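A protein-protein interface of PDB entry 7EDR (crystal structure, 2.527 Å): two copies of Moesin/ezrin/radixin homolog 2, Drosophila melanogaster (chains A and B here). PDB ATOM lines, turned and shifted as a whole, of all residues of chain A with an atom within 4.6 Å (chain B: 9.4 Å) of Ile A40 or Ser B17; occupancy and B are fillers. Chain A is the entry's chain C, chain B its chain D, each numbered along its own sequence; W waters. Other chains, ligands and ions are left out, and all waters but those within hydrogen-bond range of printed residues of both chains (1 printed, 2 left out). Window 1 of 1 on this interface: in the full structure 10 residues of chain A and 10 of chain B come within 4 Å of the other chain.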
ATOM      1  N   HIS A  19     -15.395  -6.706   5.644  1.00  0.00           N
ATOM      2  CA  HIS A  19     -16.775  -6.456   6.023  1.00  0.00           C
ATOM      3  C   HIS A  19     -17.631  -6.004   4.844  1.00  0.00           C
ATOM      4  O   HIS A  19     -17.139  -5.626   3.776  1.00  0.00           O
ATOM      5  CB  HIS A  19     -16.833  -5.441   7.159  1.00  0.00           C
ATOM      6  CG  HIS A  19     -16.266  -4.102   6.817  1.00  0.00           C
ATOM      7  ND1 HIS A  19     -15.028  -3.685   7.262  1.00  0.00           N
ATOM      8  CD2 HIS A  19     -16.787  -3.066   6.115  1.00  0.00           C
ATOM      9  CE1 HIS A  19     -14.808  -2.450   6.842  1.00  0.00           C
ATOM     10  NE2 HIS A  19     -15.861  -2.050   6.150  1.00  0.00           N
ATOM     11  N   TYR A  20     -18.943  -6.058   5.082  1.00  0.00           N
ATOM     12  CA  TYR A  20     -19.988  -5.648   4.152  1.00  0.00           C
ATOM     13  C   TYR A  20     -20.557  -4.313   4.596  1.00  0.00           C
ATOM     14  O   TYR A  20     -20.937  -4.150   5.764  1.00  0.00           O
ATOM     15  CB  TYR A  20     -21.104  -6.690   4.110  1.00  0.00           C
ATOM     16  CG  TYR A  20     -20.649  -8.029   3.601  1.00  0.00           C
ATOM     17  CD1 TYR A  20     -20.750  -8.346   2.245  1.00  0.00           C
ATOM     18  CD2 TYR A  20     -20.130  -8.988   4.465  1.00  0.00           C
ATOM     19  CE1 TYR A  20     -20.332  -9.561   1.763  1.00  0.00           C
ATOM     20  CE2 TYR A  20     -19.711 -10.226   3.986  1.00  0.00           C
ATOM     21  CZ  TYR A  20     -19.816 -10.498   2.637  1.00  0.00           C
ATOM     22  OH  TYR A  20     -19.403 -11.697   2.148  1.00  0.00           O
ATOM     23  N   LEU A  21     -20.617  -3.361   3.683  1.00  0.00           N
ATOM     24  CA  LEU A  21     -21.190  -2.055   3.986  1.00  0.00           C
ATOM     25  C   LEU A  21     -22.600  -2.003   3.404  1.00  0.00           C
ATOM     26  O   LEU A  21     -22.781  -2.191   2.196  1.00  0.00           O
ATOM     27  CB  LEU A  21     -20.315  -0.922   3.436  1.00  0.00           C
ATOM     28  CG  LEU A  21     -20.830   0.497   3.721  1.00  0.00           C
ATOM     29  CD1 LEU A  21     -21.012   0.750   5.198  1.00  0.00           C
ATOM     30  CD2 LEU A  21     -19.956   1.573   3.134  1.00  0.00           C
ATOM     31  N   PHE A  39     -25.386   0.107   8.263  1.00  0.00           N
ATOM     32  CA  PHE A  39     -24.715  -0.774   9.206  1.00  0.00           C
ATOM     33  C   PHE A  39     -23.639  -1.564   8.470  1.00  0.00           C
ATOM     34  O   PHE A  39     -23.546  -1.544   7.240  1.00  0.00           O
ATOM     35  CB  PHE A  39     -25.714  -1.704   9.908  1.00  0.00           C
ATOM     36  CG  PHE A  39     -26.578  -2.507   8.964  1.00  0.00           C
ATOM     37  CD1 PHE A  39     -26.187  -3.777   8.548  1.00  0.00           C
ATOM     38  CD2 PHE A  39     -27.793  -1.995   8.501  1.00  0.00           C
ATOM     39  CE1 PHE A  39     -26.997  -4.531   7.673  1.00  0.00           C
ATOM     40  CE2 PHE A  39     -28.602  -2.730   7.628  1.00  0.00           C
ATOM     41  CZ  PHE A  39     -28.206  -3.998   7.200  1.00  0.00           C
ATOM     42  N   ILE A  40     -22.820  -2.263   9.238  1.00  0.00           N
ATOM     43  CA  ILE A  40     -21.705  -3.016   8.694  1.00  0.00           C
ATOM     44  C   ILE A  40     -21.726  -4.395   9.327  1.00  0.00           C
ATOM     45  O   ILE A  40     -22.001  -4.528  10.524  1.00  0.00           O
ATOM     46  CB  ILE A  40     -20.370  -2.280   8.939  1.00  0.00           C
ATOM     47  CG1 ILE A  40     -20.358  -0.974   8.127  1.00  0.00           C
ATOM     48  CG2 ILE A  40     -19.160  -3.159   8.613  1.00  0.00           C
ATOM     49  CD1 ILE A  40     -19.084  -0.146   8.272  1.00  0.00           C
ATOM     50  N   LEU A  41     -21.473  -5.425   8.517  1.00  0.00           N
ATOM     51  CA  LEU A  41     -21.418  -6.807   8.987  1.00  0.00           C
ATOM     52  C   LEU A  41     -20.056  -7.377   8.626  1.00  0.00           C
ATOM     53  O   LEU A  41     -19.682  -7.392   7.448  1.00  0.00           O
ATOM     54  CB  LEU A  41     -22.544  -7.643   8.371  1.00  0.00           C
ATOM     55  CG  LEU A  41     -23.947  -7.419   8.971  1.00  0.00           C
ATOM     56  CD1 LEU A  41     -25.023  -8.104   8.152  1.00  0.00           C
ATOM     57  CD2 LEU A  41     -23.989  -7.903  10.420  1.00  0.00           C
ATOM     58  N   THR A  42     -19.308  -7.821   9.634  1.00  0.00           N
ATOM     59  CA  THR A  42     -18.024  -8.448   9.356  1.00  0.00           C
ATOM     60  C   THR A  42     -18.235  -9.784   8.660  1.00  0.00           C
ATOM     61  O   THR A  42     -19.289 -10.404   8.778  1.00  0.00           O
ATOM     62  CB  THR A  42     -17.233  -8.683  10.638  1.00  0.00           C
ATOM     63  OG1 THR A  42     -17.897  -9.689  11.407  1.00  0.00           O
ATOM     64  CG2 THR A  42     -17.098  -7.413  11.454  1.00  0.00           C
ATOM     65  N   GLU A  45     -19.290 -12.288  11.283  1.00  0.00           N
ATOM     66  CA  GLU A  45     -20.704 -12.198  11.630  1.00  0.00           C
ATOM     67  C   GLU A  45     -21.556 -12.927  10.596  1.00  0.00           C
ATOM     68  O   GLU A  45     -22.451 -13.700  10.946  1.00  0.00           O
ATOM     69  CB  GLU A  45     -21.136 -10.740  11.745  1.00  0.00           C
ATOM     70  CG  GLU A  45     -20.654 -10.036  13.001  1.00  0.00           C
ATOM     71  CD  GLU A  45     -21.157  -8.605  13.067  1.00  0.00           C
ATOM     72  OE1 GLU A  45     -20.748  -7.786  12.210  1.00  0.00           O
ATOM     73  OE2 GLU A  45     -21.982  -8.308  13.955  1.00  0.00           O
ATOM     74  N   THR B  14     -20.212   9.014  -4.694  1.00  0.00           N
ATOM     75  CA  THR B  14     -19.333   8.780  -3.554  1.00  0.00           C
ATOM     76  C   THR B  14     -19.898   7.704  -2.630  1.00  0.00           C
ATOM     77  O   THR B  14     -21.075   7.750  -2.251  1.00  0.00           O
ATOM     78  CB  THR B  14     -19.130  10.072  -2.754  1.00  0.00           C
ATOM     79  OG1 THR B  14     -18.591  11.099  -3.594  1.00  0.00           O
ATOM     80  CG2 THR B  14     -18.186   9.839  -1.583  1.00  0.00           C
ATOM     81  N   THR B  15     -19.050   6.750  -2.249  1.00  0.00           N
ATOM     82  CA  THR B  15     -19.321   5.850  -1.134  1.00  0.00           C
ATOM     83  C   THR B  15     -18.388   6.232   0.007  1.00  0.00           C
ATOM     84  O   THR B  15     -17.165   6.106  -0.117  1.00  0.00           O
ATOM     85  CB  THR B  15     -19.109   4.382  -1.530  1.00  0.00           C
ATOM     86  OG1 THR B  15     -20.066   3.991  -2.521  1.00  0.00           O
ATOM     87  CG2 THR B  15     -19.237   3.464  -0.314  1.00  0.00           C
ATOM     88  N   HIS B  16     -18.945   6.686   1.114  1.00  0.00           N
ATOM     89  CA  HIS B  16     -18.139   7.067   2.267  1.00  0.00           C
ATOM     90  C   HIS B  16     -18.601   6.295   3.499  1.00  0.00           C
ATOM     91  O   HIS B  16     -19.797   6.077   3.698  1.00  0.00           O
ATOM     92  CB  HIS B  16     -18.204   8.582   2.521  1.00  0.00           C
ATOM     93  CG  HIS B  16     -17.334   9.036   3.654  1.00  0.00           C
ATOM     94  ND1 HIS B  16     -17.789   9.123   4.953  1.00  0.00           N
ATOM     95  CD2 HIS B  16     -16.032   9.409   3.687  1.00  0.00           C
ATOM     96  CE1 HIS B  16     -16.805   9.534   5.734  1.00  0.00           C
ATOM     97  NE2 HIS B  16     -15.729   9.713   4.994  1.00  0.00           N
ATOM     98  N   SER B  17     -17.650   5.881   4.321  1.00  0.00           N
ATOM     99  CA  SER B  17     -17.943   5.092   5.503  1.00  0.00           C
ATOM    100  C   SER B  17     -17.208   5.679   6.699  1.00  0.00           C
ATOM    101  O   SER B  17     -16.015   5.998   6.620  1.00  0.00           O
ATOM    102  CB  SER B  17     -17.543   3.622   5.313  1.00  0.00           C
ATOM    103  OG  SER B  17     -17.813   2.868   6.498  1.00  0.00           O
ATOM    104  N   SER B  18     -17.921   5.805   7.807  1.00  0.00           N
ATOM    105  CA  SER B  18     -17.361   6.317   9.046  1.00  0.00           C
ATOM    106  C   SER B  18     -17.814   5.364  10.135  1.00  0.00           C
ATOM    107  O   SER B  18     -19.023   5.188  10.326  1.00  0.00           O
ATOM    108  CB  SER B  18     -17.858   7.743   9.303  1.00  0.00           C
ATOM    109  OG  SER B  18     -16.867   8.529   9.930  1.00  0.00           O
ATOM    110  N   HIS B  19     -16.866   4.722  10.821  1.00  0.00           N
ATOM    111  CA  HIS B  19     -17.261   3.644  11.721  1.00  0.00           C
ATOM    112  C   HIS B  19     -16.168   3.329  12.742  1.00  0.00           C
ATOM    113  O   HIS B  19     -15.006   3.735  12.602  1.00  0.00           O
ATOM    114  CB  HIS B  19     -17.624   2.381  10.932  1.00  0.00           C
ATOM    115  CG  HIS B  19     -16.490   1.823  10.129  1.00  0.00           C
ATOM    116  ND1 HIS B  19     -16.434   1.920   8.755  1.00  0.00           N
ATOM    117  CD2 HIS B  19     -15.364   1.166  10.507  1.00  0.00           C
ATOM    118  CE1 HIS B  19     -15.328   1.342   8.318  1.00  0.00           C
ATOM    119  NE2 HIS B  19     -14.657   0.886   9.362  1.00  0.00           N
ATOM    120  N   TYR B  20     -16.572   2.576  13.768  1.00  0.00           N
ATOM    121  CA  TYR B  20     -15.705   2.132  14.854  1.00  0.00           C
ATOM    122  C   TYR B  20     -15.429   0.645  14.694  1.00  0.00           C
ATOM    123  O   TYR B  20     -16.366  -0.131  14.510  1.00  0.00           O
ATOM    124  CB  TYR B  20     -16.361   2.400  16.218  1.00  0.00           C
ATOM    125  CG  TYR B  20     -16.628   3.860  16.499  1.00  0.00           C
ATOM    126  CD1 TYR B  20     -17.802   4.468  16.074  1.00  0.00           C
ATOM    127  CD2 TYR B  20     -15.698   4.635  17.170  1.00  0.00           C
ATOM    128  CE1 TYR B  20     -18.051   5.813  16.325  1.00  0.00           C
ATOM    129  CE2 TYR B  20     -15.931   5.983  17.421  1.00  0.00           C
ATOM    130  CZ  TYR B  20     -17.115   6.568  17.001  1.00  0.00           C
ATOM    131  OH  TYR B  20     -17.341   7.905  17.253  1.00  0.00           O
ATOM    132  N   LEU B  21     -14.157   0.250  14.740  1.00  0.00           N
ATOM    133  CA  LEU B  21     -13.784  -1.158  14.742  1.00  0.00           C
ATOM    134  C   LEU B  21     -13.500  -1.563  16.173  1.00  0.00           C
ATOM    135  O   LEU B  21     -12.553  -1.056  16.796  1.00  0.00           O
ATOM    136  CB  LEU B  21     -12.557  -1.476  13.887  1.00  0.00           C
ATOM    137  CG  LEU B  21     -12.368  -0.949  12.475  1.00  0.00           C
ATOM    138  CD1 LEU B  21     -10.931  -1.178  12.063  1.00  0.00           C
ATOM    139  CD2 LEU B  21     -13.302  -1.644  11.489  1.00  0.00           C
ATOM    140  N   PRO B  36     -20.414 -11.164  19.339  1.00  0.00           N
ATOM    141  CA  PRO B  36     -19.195 -11.303  18.536  1.00  0.00           C
ATOM    142  C   PRO B  36     -17.976 -10.639  19.190  1.00  0.00           C
ATOM    143  O   PRO B  36     -18.110  -9.604  19.836  1.00  0.00           O
ATOM    144  CB  PRO B  36     -19.564 -10.603  17.224  1.00  0.00           C
ATOM    145  CG  PRO B  36     -20.573  -9.564  17.621  1.00  0.00           C
ATOM    146  CD  PRO B  36     -21.299 -10.095  18.828  1.00  0.00           C
ATOM    147  N   GLU B  38     -15.388  -9.477  17.496  1.00  0.00           N
ATOM    148  CA  GLU B  38     -15.075  -8.369  16.605  1.00  0.00           C
ATOM    149  C   GLU B  38     -16.375  -7.853  16.014  1.00  0.00           C
ATOM    150  O   GLU B  38     -17.214  -8.650  15.569  1.00  0.00           O
ATOM    151  CB  GLU B  38     -14.116  -8.791  15.484  1.00  0.00           C
ATOM    152  CG  GLU B  38     -12.847  -9.500  15.980  1.00  0.00           C
ATOM    153  CD  GLU B  38     -11.882  -9.941  14.858  1.00  0.00           C
ATOM    154  OE1 GLU B  38     -12.353 -10.299  13.743  1.00  0.00           O
ATOM    155  OE2 GLU B  38     -10.648  -9.938  15.110  1.00  0.00           O
ATOM    156  N   PHE B  39     -16.551  -6.528  16.023  1.00  0.00           N
ATOM    157  CA  PHE B  39     -17.728  -5.925  15.403  1.00  0.00           C
ATOM    158  C   PHE B  39     -17.419  -4.474  15.034  1.00  0.00           C
ATOM    159  O   PHE B  39     -16.426  -3.883  15.463  1.00  0.00           O
ATOM    160  CB  PHE B  39     -18.990  -6.038  16.300  1.00  0.00           C
ATOM    161  CG  PHE B  39     -18.834  -5.418  17.672  1.00  0.00           C
ATOM    162  CD1 PHE B  39     -18.253  -6.134  18.720  1.00  0.00           C
ATOM    163  CD2 PHE B  39     -19.256  -4.108  17.914  1.00  0.00           C
ATOM    164  CE1 PHE B  39     -18.094  -5.564  19.989  1.00  0.00           C
ATOM    165  CE2 PHE B  39     -19.107  -3.528  19.183  1.00  0.00           C
ATOM    166  CZ  PHE B  39     -18.522  -4.266  20.223  1.00  0.00           C
ATOM    167  N   ILE B  40     -18.290  -3.912  14.220  1.00  0.00           N
ATOM    168  CA  ILE B  40     -18.099  -2.579  13.687  1.00  0.00           C
ATOM    169  C   ILE B  40     -19.357  -1.778  13.981  1.00  0.00           C
ATOM    170  O   ILE B  40     -20.473  -2.224  13.679  1.00  0.00           O
ATOM    171  CB  ILE B  40     -17.789  -2.608  12.179  1.00  0.00           C
ATOM    172  CG1 ILE B  40     -16.418  -3.242  11.957  1.00  0.00           C
ATOM    173  CG2 ILE B  40     -17.845  -1.193  11.607  1.00  0.00           C
ATOM    174  CD1 ILE B  40     -16.065  -3.538  10.505  1.00  0.00           C
ATOM    175  N   LEU B  41     -19.179  -0.614  14.600  1.00  0.00           N
ATOM    176  CA  LEU B  41     -20.281   0.290  14.897  1.00  0.00           C
ATOM    177  C   LEU B  41     -20.143   1.509  14.011  1.00  0.00           C
ATOM    178  O   LEU B  41     -19.165   2.258  14.099  1.00  0.00           O
ATOM    179  CB  LEU B  41     -20.314   0.706  16.361  1.00  0.00           C
ATOM    180  CG  LEU B  41     -20.818  -0.389  17.287  1.00  0.00           C
ATOM    181  CD1 LEU B  41     -20.402  -0.025  18.680  1.00  0.00           C
ATOM    182  CD2 LEU B  41     -22.307  -0.493  17.187  1.00  0.00           C
ATOM    183  N   THR B  42     -21.123   1.687  13.163  1.00  0.00           N
ATOM    184  CA  THR B  42     -21.199   2.823  12.285  1.00  0.00           C
ATOM    185  C   THR B  42     -21.454   4.101  13.087  1.00  0.00           C
ATOM    186  O   THR B  42     -22.025   4.064  14.180  1.00  0.00           O
ATOM    187  CB  THR B  42     -22.301   2.508  11.292  1.00  0.00           C
ATOM    188  OG1 THR B  42     -21.801   2.624   9.963  1.00  0.00           O
ATOM    189  CG2 THR B  42     -23.482   3.334  11.521  1.00  0.00           C
ATOM    190  N   ASP B  43     -20.987   5.237  12.553  1.00  0.00           N
ATOM    191  CA  ASP B  43     -21.226   6.535  13.191  1.00  0.00           C
ATOM    192  C   ASP B  43     -22.709   6.763  13.467  1.00  0.00           C
ATOM    193  O   ASP B  43     -23.087   7.226  14.552  1.00  0.00           O
ATOM    194  CB  ASP B  43     -20.712   7.681  12.317  1.00  0.00           C
ATOM    195  CG  ASP B  43     -19.259   8.065  12.602  1.00  0.00           C
ATOM    196  OD1 ASP B  43     -18.486   7.245  13.141  1.00  0.00           O
ATOM    197  OD2 ASP B  43     -18.876   9.205  12.251  1.00  0.00           O
ATOM    198  N   ASN B  44     -23.570   6.496  12.476  1.00  0.00           N
ATOM    199  CA  ASN B  44     -24.972   6.832  12.685  1.00  0.00           C
ATOM    200  C   ASN B  44     -25.616   5.893  13.693  1.00  0.00           C
ATOM    201  O   ASN B  44     -26.492   6.324  14.451  1.00  0.00           O
ATOM    202  CB  ASN B  44     -25.762   6.883  11.361  1.00  0.00           C
ATOM    203  CG  ASN B  44     -26.084   5.506  10.780  1.00  0.00           C
ATOM    204  OD1 ASN B  44     -25.276   4.934  10.058  1.00  0.00           O
ATOM    205  ND2 ASN B  44     -27.289   4.984  11.065  1.00  0.00           N
ATOM    206  N   GLU B  45     -25.176   4.631  13.749  1.00  0.00           N
ATOM    207  CA  GLU B  45     -25.597   3.752  14.830  1.00  0.00           C
ATOM    208  C   GLU B  45     -25.249   4.365  16.177  1.00  0.00           C
ATOM    209  O   GLU B  45     -26.096   4.431  17.073  1.00  0.00           O
ATOM    210  CB  GLU B  45     -24.959   2.365  14.701  1.00  0.00           C
ATOM    211  CG  GLU B  45     -25.708   1.396  13.815  1.00  0.00           C
ATOM    212  CD  GLU B  45     -24.935   0.097  13.596  1.00  0.00           C
ATOM    213  OE1 GLU B  45     -25.374  -0.976  14.080  1.00  0.00           O
ATOM    214  OE2 GLU B  45     -23.861   0.153  12.960  1.00  0.00           O
HETATM  215  O   HOH W   1     -20.491  -5.200  13.005  1.00  0.00           O
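Water W1 lies within hydrogen-bond range of OE1 of Glu A45 (2.7 Å), N of Ile B40 (2.8 Å) and O of Ile A40 (3.0 Å).
Of the printed residues of chain B, His A19 touches Ile B40. Tyr A20 touches none of the printed residues of chain B. Of the printed residues of chain B, Phe A39 touches Glu B45. Of chain B, only Ser B17 (3.7 Å), His B19 (3.4 Å) and Ile B40 (3.6 Å) come within 4 Å of Ile A40. No residue of chain B comes within 4 Å of Leu A41. Of chain A, only Leu A21 (3.8 Å) and Ile A40 (3.7 Å) come within 4 Å of Ser B17. Of the printed residues of chain A, Ile B40 touches His A19 and Ile A40. Printed residues of chain A within 4 Å of Glu B45: Phe A39 (3.96 Å). The nearest residue of chain B that does not touch Ile A40 is Thr B42 (4.2 Å).
Of the 8 printed residues of chain A, 4 touch a printed residue of chain B. Printed residues of chain A that touch a printed residue of chain B: His A19, Leu A21, Phe A39 and Ile A40. Hydrophobic or aromatic side chains of chain A within 4 Å of the printed part of chain B: His A19, Leu A21 and Ile A40. Hydrophobic or aromatic side chains of chain B that line the printed part of chain A: His B19 and Ile B40. Among the printed residues, 7 pairs touch across the chains. Among the printed residues, no Asp or Glu carboxylate lies within 4 Å of a Lys or Arg side-chain nitrogen of the other chain.
OG of Ser B17 is in hydrogen-bond range of ND1 of His B19. N of Thr B42 is in hydrogen-bond range of OE2 of Glu B45 (3.1 Å).
CD1 of Ile B40 touches ND1 of His A19, at 3.4 Å. Leu A21 touches Thr B15 (CD2 to CG2, 3.998 Å). Leu A21 touches Ser B17 (CD2 to CB, 3.8 Å). Phe A39 touches Glu B45. Ser B17 touches Ile A40 (OG to CD1, 3.7 Å). His B19 touches Ile A40 (ND1 to CD1, 3.4 Å). Ile B40 touches Ile A40 (CD1 to CG2, 3.6 Å).
His A19 touches Ile B40, and with the chains exchanged Ile A40 touches His B19. Phe A39 touches Glu B45, but with the chains exchanged Glu A45 does not touch Phe B39 (4.4 Å). Ile B40 touches its own counterpart, Ile A40. Of the 7 pairs that touch across the chains among the printed residues, 3 have their exchanged pair printed and touching as well.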
